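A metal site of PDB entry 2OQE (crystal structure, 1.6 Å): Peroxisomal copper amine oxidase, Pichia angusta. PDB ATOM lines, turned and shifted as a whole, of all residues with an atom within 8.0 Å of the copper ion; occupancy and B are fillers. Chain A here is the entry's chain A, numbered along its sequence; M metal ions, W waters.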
ATOM      1  N   VAL A 291      11.941  -0.873  27.535  1.00  0.00           N
ATOM      2  CA  VAL A 291      11.177  -0.091  26.576  1.00  0.00           C
ATOM      3  C   VAL A 291       9.681  -0.292  26.918  1.00  0.00           C
ATOM      4  O   VAL A 291       8.979  -1.079  26.237  1.00  0.00           O
ATOM      5  CB  VAL A 291      11.545  -0.503  25.140  1.00  0.00           C
ATOM      6  CG1 VAL A 291      10.800   0.344  24.073  1.00  0.00           C
ATOM      7  CG2 VAL A 291      13.102  -0.395  24.940  1.00  0.00           C
ATOM      8  N   TYR A 293       5.789   0.027  27.259  1.00  0.00           N
ATOM      9  CA  TYR A 293       4.642   0.570  26.557  1.00  0.00           C
ATOM     10  C   TYR A 293       3.594   1.084  27.530  1.00  0.00           C
ATOM     11  O   TYR A 293       3.518   0.642  28.682  1.00  0.00           O
ATOM     12  CB  TYR A 293       4.088  -0.473  25.580  1.00  0.00           C
ATOM     13  CG  TYR A 293       4.915  -0.478  24.314  1.00  0.00           C
ATOM     14  CD1 TYR A 293       4.457   0.114  23.134  1.00  0.00           C
ATOM     15  CD2 TYR A 293       6.208  -1.022  24.323  1.00  0.00           C
ATOM     16  CE1 TYR A 293       5.261   0.135  21.975  1.00  0.00           C
ATOM     17  CE2 TYR A 293       7.011  -1.030  23.167  1.00  0.00           C
ATOM     18  CZ  TYR A 293       6.541  -0.433  22.021  1.00  0.00           C
ATOM     19  OH  TYR A 293       7.367  -0.436  20.912  1.00  0.00           O
ATOM     20  N   ASN A 392      11.479  -4.959  15.557  1.00  0.00           N
ATOM     21  CA  ASN A 392      11.123  -3.772  14.812  1.00  0.00           C
ATOM     22  C   ASN A 392      12.094  -2.621  15.041  1.00  0.00           C
ATOM     23  O   ASN A 392      12.249  -1.780  14.148  1.00  0.00           O
ATOM     24  CB  ASN A 392       9.703  -3.324  15.183  1.00  0.00           C
ATOM     25  CG  ASN A 392       9.531  -3.141  16.672  1.00  0.00           C
ATOM     26  OD1 ASN A 392       9.484  -4.118  17.409  1.00  0.00           O
ATOM     27  ND2 ASN A 392       9.447  -1.895  17.120  1.00  0.00           N
ATOM     28  N   TPQ A 393      12.793  -2.468  16.100  1.00  0.00           N
ATOM     29  CA  TPQ A 393      13.652  -1.402  16.640  1.00  0.00           C
ATOM     30  CB  TPQ A 393      13.917  -1.476  18.165  1.00  0.00           C
ATOM     31  C   TPQ A 393      14.990  -1.450  15.935  1.00  0.00           C
ATOM     32  O   TPQ A 393      15.623  -2.522  16.030  1.00  0.00           O
ATOM     33  C1  TPQ A 393      12.709  -1.522  19.078  1.00  0.00           C
ATOM     34  C2  TPQ A 393      11.701  -0.427  19.088  1.00  0.00           C
ATOM     35  O2  TPQ A 393      11.832   0.634  18.255  1.00  0.00           O
ATOM     36  C3  TPQ A 393      10.598  -0.495  19.936  1.00  0.00           C
ATOM     37  C4  TPQ A 393      10.450  -1.575  20.786  1.00  0.00           C
ATOM     38  O4  TPQ A 393       9.386  -1.675  21.628  1.00  0.00           O
ATOM     39  C5  TPQ A 393      11.446  -2.665  20.810  1.00  0.00           C
ATOM     40  O5  TPQ A 393      11.255  -3.699  21.686  1.00  0.00           O
ATOM     41  C6  TPQ A 393      12.553  -2.610  19.942  1.00  0.00           C
ATOM     42  N   TYR A 395      18.767   0.372  16.940  1.00  0.00           N
ATOM     43  CA  TYR A 395      19.509   1.259  17.837  1.00  0.00           C
ATOM     44  C   TYR A 395      20.905   1.401  17.278  1.00  0.00           C
ATOM     45  O   TYR A 395      21.656   0.434  17.203  1.00  0.00           O
ATOM     46  CB  TYR A 395      19.566   0.690  19.263  1.00  0.00           C
ATOM     47  CG  TYR A 395      18.231   0.553  19.940  1.00  0.00           C
ATOM     48  CD1 TYR A 395      17.664   1.638  20.598  1.00  0.00           C
ATOM     49  CD2 TYR A 395      17.514  -0.656  19.914  1.00  0.00           C
ATOM     50  CE1 TYR A 395      16.412   1.543  21.227  1.00  0.00           C
ATOM     51  CE2 TYR A 395      16.276  -0.769  20.563  1.00  0.00           C
ATOM     52  CZ  TYR A 395      15.739   0.344  21.209  1.00  0.00           C
ATOM     53  OH  TYR A 395      14.519   0.274  21.878  1.00  0.00           O
ATOM     54  N   LEU A 413      17.813   6.321  17.356  1.00  0.00           N
ATOM     55  CA  LEU A 413      16.742   5.353  17.264  1.00  0.00           C
ATOM     56  C   LEU A 413      16.113   5.437  15.895  1.00  0.00           C
ATOM     57  O   LEU A 413      15.722   6.514  15.445  1.00  0.00           O
ATOM     58  CB  LEU A 413      15.655   5.634  18.300  1.00  0.00           C
ATOM     59  CG  LEU A 413      15.995   5.813  19.771  1.00  0.00           C
ATOM     60  CD1 LEU A 413      14.736   6.037  20.588  1.00  0.00           C
ATOM     61  CD2 LEU A 413      16.785   4.658  20.305  1.00  0.00           C
ATOM     62  N   THR A 414      16.004   4.296  15.232  1.00  0.00           N
ATOM     63  CA  THR A 414      15.290   4.216  13.970  1.00  0.00           C
ATOM     64  C   THR A 414      14.569   2.857  13.881  1.00  0.00           C
ATOM     65  O   THR A 414      14.219   2.274  14.926  1.00  0.00           O
ATOM     66  CB  THR A 414      16.202   4.599  12.744  1.00  0.00           C
ATOM     67  OG1 THR A 414      15.444   4.554  11.509  1.00  0.00           O
ATOM     68  CG2 THR A 414      17.449   3.710  12.655  1.00  0.00           C
ATOM     69  N   ILE A 416      11.237   0.589  12.946  1.00  0.00           N
ATOM     70  CA  ILE A 416       9.809   0.650  12.714  1.00  0.00           C
ATOM     71  C   ILE A 416       9.072   0.672  14.049  1.00  0.00           C
ATOM     72  O   ILE A 416       9.455   0.007  14.987  1.00  0.00           O
ATOM     73  CB  ILE A 416       9.380  -0.537  11.818  1.00  0.00           C
ATOM     74  CG1 ILE A 416      10.121  -0.421  10.465  1.00  0.00           C
ATOM     75  CG2 ILE A 416       7.854  -0.516  11.576  1.00  0.00           C
ATOM     76  CD1 ILE A 416       9.849  -1.533   9.476  1.00  0.00           C
ATOM     77  N   LEU A 417       7.994   1.451  14.098  1.00  0.00           N
ATOM     78  CA  LEU A 417       7.082   1.411  15.247  1.00  0.00           C
ATOM     79  C   LEU A 417       6.480   0.023  15.475  1.00  0.00           C
ATOM     80  O   LEU A 417       6.069  -0.637  14.524  1.00  0.00           O
ATOM     81  CB  LEU A 417       5.927   2.387  15.029  1.00  0.00           C
ATOM     82  CG  LEU A 417       6.279   3.871  14.936  1.00  0.00           C
ATOM     83  CD1 LEU A 417       5.026   4.597  14.508  1.00  0.00           C
ATOM     84  CD2 LEU A 417       6.794   4.392  16.285  1.00  0.00           C
ATOM     85  N   ASN A 418       6.448  -0.428  16.721  1.00  0.00           N
ATOM     86  CA  ASN A 418       5.619  -1.584  17.060  1.00  0.00           C
ATOM     87  C   ASN A 418       4.169  -1.123  16.937  1.00  0.00           C
ATOM     88  O   ASN A 418       3.804  -0.072  17.463  1.00  0.00           O
ATOM     89  CB  ASN A 418       5.903  -2.079  18.470  1.00  0.00           C
ATOM     90  CG  ASN A 418       4.828  -3.025  18.970  1.00  0.00           C
ATOM     91  OD1 ASN A 418       3.843  -2.587  19.552  1.00  0.00           O
ATOM     92  ND2 ASN A 418       4.991  -4.311  18.684  1.00  0.00           N
ATOM     93  N   HIS A 442       1.392   2.323  19.881  1.00  0.00           N
ATOM     94  CA  HIS A 442       1.273   2.667  21.304  1.00  0.00           C
ATOM     95  C   HIS A 442       2.423   3.531  21.816  1.00  0.00           C
ATOM     96  O   HIS A 442       3.571   3.410  21.358  1.00  0.00           O
ATOM     97  CB  HIS A 442       1.239   1.394  22.161  1.00  0.00           C
ATOM     98  CG  HIS A 442      -0.012   0.583  22.011  1.00  0.00           C
ATOM     99  ND1 HIS A 442      -0.018  -0.793  22.062  1.00  0.00           N
ATOM    100  CD2 HIS A 442      -1.300   0.959  21.815  1.00  0.00           C
ATOM    101  CE1 HIS A 442      -1.249  -1.241  21.910  1.00  0.00           C
ATOM    102  NE2 HIS A 442      -2.052  -0.193  21.759  1.00  0.00           N
ATOM    103  N   ASN A 443       2.100   4.383  22.796  1.00  0.00           N
ATOM    104  CA  ASN A 443       3.094   5.180  23.525  1.00  0.00           C
ATOM    105  C   ASN A 443       4.083   4.230  24.188  1.00  0.00           C
ATOM    106  O   ASN A 443       3.718   3.154  24.667  1.00  0.00           O
ATOM    107  CB  ASN A 443       2.378   5.950  24.649  1.00  0.00           C
ATOM    108  CG  ASN A 443       1.342   6.949  24.117  1.00  0.00           C
ATOM    109  OD1 ASN A 443       1.328   7.276  22.920  1.00  0.00           O
ATOM    110  ND2 ASN A 443       0.498   7.471  25.036  1.00  0.00           N
ATOM    111  N   HIS A 444       5.345   4.666  24.260  1.00  0.00           N
ATOM    112  CA  HIS A 444       6.338   3.856  24.987  1.00  0.00           C
ATOM    113  C   HIS A 444       7.501   4.767  25.334  1.00  0.00           C
ATOM    114  O   HIS A 444       7.662   5.832  24.742  1.00  0.00           O
ATOM    115  CB  HIS A 444       6.820   2.685  24.134  1.00  0.00           C
ATOM    116  CG  HIS A 444       7.300   3.101  22.787  1.00  0.00           C
ATOM    117  ND1 HIS A 444       6.431   3.431  21.759  1.00  0.00           N
ATOM    118  CD2 HIS A 444       8.550   3.276  22.293  1.00  0.00           C
ATOM    119  CE1 HIS A 444       7.135   3.791  20.695  1.00  0.00           C
ATOM    120  NE2 HIS A 444       8.424   3.713  20.996  1.00  0.00           N
ATOM    121  N   GLN A 445       8.319   4.330  26.306  1.00  0.00           N
ATOM    122  CA  GLN A 445       9.590   5.009  26.603  1.00  0.00           C
ATOM    123  C   GLN A 445      10.714   4.077  26.114  1.00  0.00           C
ATOM    124  O   GLN A 445      10.501   2.873  25.998  1.00  0.00           O
ATOM    125  CB  GLN A 445       9.753   5.226  28.105  1.00  0.00           C
ATOM    126  CG  GLN A 445       8.646   6.046  28.730  1.00  0.00           C
ATOM    127  CD  GLN A 445       8.939   6.405  30.179  1.00  0.00           C
ATOM    128  OE1 GLN A 445       8.685   5.598  31.082  1.00  0.00           O
ATOM    129  NE2 GLN A 445       9.446   7.616  30.395  1.00  0.00           N
ATOM    130  N   HIS A 446      11.893   4.645  25.826  1.00  0.00           N
ATOM    131  CA  HIS A 446      13.111   3.854  25.637  1.00  0.00           C
ATOM    132  C   HIS A 446      14.053   4.319  26.727  1.00  0.00           C
ATOM    133  O   HIS A 446      14.470   5.470  26.724  1.00  0.00           O
ATOM    134  CB  HIS A 446      13.802   4.125  24.296  1.00  0.00           C
ATOM    135  CG  HIS A 446      12.948   3.874  23.093  1.00  0.00           C
ATOM    136  ND1 HIS A 446      13.062   2.724  22.333  1.00  0.00           N
ATOM    137  CD2 HIS A 446      12.005   4.640  22.495  1.00  0.00           C
ATOM    138  CE1 HIS A 446      12.201   2.793  21.317  1.00  0.00           C
ATOM    139  NE2 HIS A 446      11.566   3.951  21.399  1.00  0.00           N
ATOM    140  N   ILE A 610      14.322   8.347  26.250  1.00  0.00           N
ATOM    141  CA  ILE A 610      13.285   9.213  25.705  1.00  0.00           C
ATOM    142  C   ILE A 610      11.880   8.654  25.957  1.00  0.00           C
ATOM    143  O   ILE A 610      11.725   7.464  26.230  1.00  0.00           O
ATOM    144  CB  ILE A 610      13.428   9.438  24.168  1.00  0.00           C
ATOM    145  CG1 ILE A 610      13.346   8.121  23.408  1.00  0.00           C
ATOM    146  CG2 ILE A 610      14.730  10.180  23.835  1.00  0.00           C
ATOM    147  CD1 ILE A 610      12.677   8.217  22.038  1.00  0.00           C
ATOM    148  N   THR A 611      10.877   9.523  25.871  1.00  0.00           N
ATOM    149  CA  THR A 611       9.482   9.102  25.883  1.00  0.00           C
ATOM    150  C   THR A 611       8.917   9.363  24.484  1.00  0.00           C
ATOM    151  O   THR A 611       9.026  10.469  23.963  1.00  0.00           O
ATOM    152  CB  THR A 611       8.691   9.887  26.952  1.00  0.00           C
ATOM    153  OG1 THR A 611       9.270   9.650  28.240  1.00  0.00           O
ATOM    154  CG2 THR A 611       7.246   9.429  26.981  1.00  0.00           C
ATOM    155  N   HIS A 612       8.362   8.330  23.871  1.00  0.00           N
ATOM    156  CA  HIS A 612       7.961   8.375  22.469  1.00  0.00           C
ATOM    157  C   HIS A 612       6.441   8.332  22.348  1.00  0.00           C
ATOM    158  O   HIS A 612       5.802   7.327  22.711  1.00  0.00           O
ATOM    159  CB  HIS A 612       8.575   7.158  21.744  1.00  0.00           C
ATOM    160  CG  HIS A 612       8.460   7.213  20.245  1.00  0.00           C
ATOM    161  ND1 HIS A 612       9.110   6.315  19.426  1.00  0.00           N
ATOM    162  CD2 HIS A 612       7.778   8.054  19.434  1.00  0.00           C
ATOM    163  CE1 HIS A 612       8.841   6.599  18.166  1.00  0.00           C
ATOM    164  NE2 HIS A 612       8.050   7.655  18.146  1.00  0.00           N
ATOM    165  N   PHE A 613       5.880   9.440  21.875  1.00  0.00           N
ATOM    166  CA  PHE A 613       4.454   9.528  21.483  1.00  0.00           C
ATOM    167  C   PHE A 613       4.439   9.515  19.947  1.00  0.00           C
ATOM    168  O   PHE A 613       4.795  10.510  19.325  1.00  0.00           O
ATOM    169  CB  PHE A 613       3.814  10.804  22.050  1.00  0.00           C
ATOM    170  CG  PHE A 613       3.825  10.845  23.563  1.00  0.00           C
ATOM    171  CD1 PHE A 613       2.938  10.057  24.285  1.00  0.00           C
ATOM    172  CD2 PHE A 613       4.760  11.614  24.228  1.00  0.00           C
ATOM    173  CE1 PHE A 613       2.943  10.058  25.658  1.00  0.00           C
ATOM    174  CE2 PHE A 613       4.792  11.627  25.624  1.00  0.00           C
ATOM    175  CZ  PHE A 613       3.883  10.840  26.341  1.00  0.00           C
ATOM    176  N   PRO A 614       4.116   8.347  19.344  1.00  0.00           N
ATOM    177  CA  PRO A 614       4.249   8.230  17.887  1.00  0.00           C
ATOM    178  C   PRO A 614       3.450   9.259  17.102  1.00  0.00           C
ATOM    179  O   PRO A 614       2.390   9.709  17.546  1.00  0.00           O
ATOM    180  CB  PRO A 614       3.742   6.817  17.594  1.00  0.00           C
ATOM    181  CG  PRO A 614       4.063   6.047  18.927  1.00  0.00           C
ATOM    182  CD  PRO A 614       3.715   7.081  19.972  1.00  0.00           C
ATOM    183  N   ASP A 618       6.720   9.091  11.828  1.00  0.00           N
ATOM    184  CA  ASP A 618       7.502   7.926  12.292  1.00  0.00           C
ATOM    185  C   ASP A 618       7.194   6.687  11.476  1.00  0.00           C
ATOM    186  O   ASP A 618       7.804   5.641  11.678  1.00  0.00           O
ATOM    187  CB  ASP A 618       7.204   7.604  13.767  1.00  0.00           C
ATOM    188  CG  ASP A 618       7.561   8.730  14.721  1.00  0.00           C
ATOM    189  OD1 ASP A 618       8.477   9.538  14.438  1.00  0.00           O
ATOM    190  OD2 ASP A 618       6.902   8.793  15.780  1.00  0.00           O
ATOM    191  N   SME A 622      10.897   4.948  10.625  1.00  0.00           N
ATOM    192  CA  SME A 622      11.117   6.156  11.426  1.00  0.00           C
ATOM    193  CB  SME A 622      10.876   5.792  12.892  1.00  0.00           C
ATOM    194  CG  SME A 622      12.115   5.651  13.746  1.00  0.00           C
ATOM    195  S   SME A 622      11.531   5.410  15.461  1.00  0.00           S
ATOM    196  OE  SME A 622      10.752   3.733  15.545  1.00  0.00           O
ATOM    197  CE  SME A 622      10.688   6.929  15.496  1.00  0.00           C
ATOM    198  C   SME A 622      12.414   6.883  11.200  1.00  0.00           C
ATOM    199  O   SME A 622      13.480   6.286  11.223  1.00  0.00           O
ATOM    200  N   GLU A 625      15.983   9.351  15.621  1.00  0.00           N
ATOM    201  CA  GLU A 625      15.778  10.207  16.788  1.00  0.00           C
ATOM    202  C   GLU A 625      17.013  10.163  17.682  1.00  0.00           C
ATOM    203  O   GLU A 625      17.419   9.082  18.108  1.00  0.00           O
ATOM    204  CB  GLU A 625      14.537   9.805  17.612  1.00  0.00           C
ATOM    205  CG  GLU A 625      14.307  10.791  18.768  1.00  0.00           C
ATOM    206  CD  GLU A 625      12.961  10.689  19.475  1.00  0.00           C
ATOM    207  OE1 GLU A 625      12.085   9.935  19.001  1.00  0.00           O
ATOM    208  OE2 GLU A 625      12.798  11.384  20.517  1.00  0.00           O
HETATM  209 CU    CU M   1      10.097   4.689  20.233  1.00  0.00          CU
HETATM  210  O   HOH W   1       9.722   2.654  18.270  1.00  0.00           O
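O of Ile 610 is in hydrogen-bond range of N of His 446, at 2.9 Å.
A ring nitrogen (ND1) of His 446 is in hydrogen-bond range of the side-chain hydroxyl of Tyr 395, at 2.9 Å.
A ring nitrogen (NE2) of His 612 is in hydrogen-bond range of the side-chain carboxylate (OD2) of Asp 618.
A ring nitrogen (ND1) of His 444 lies within hydrogen-bond range of the backbone carbonyl oxygen (O) of His 442 (2.9 Å).
The copper ion is bound by a ring nitrogen (NE2) of His 446.
A ring nitrogen (ND1) of His 612 binds the copper ion (2.1 Å).
NE2 of His 444 binds the copper ion (2.1 Å).
The copper ion has three donor atoms within binding distance.
Water W1 bridges O2 of TPQ 393 (2.9 Å) and OE of SME 622 (3.1 Å).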
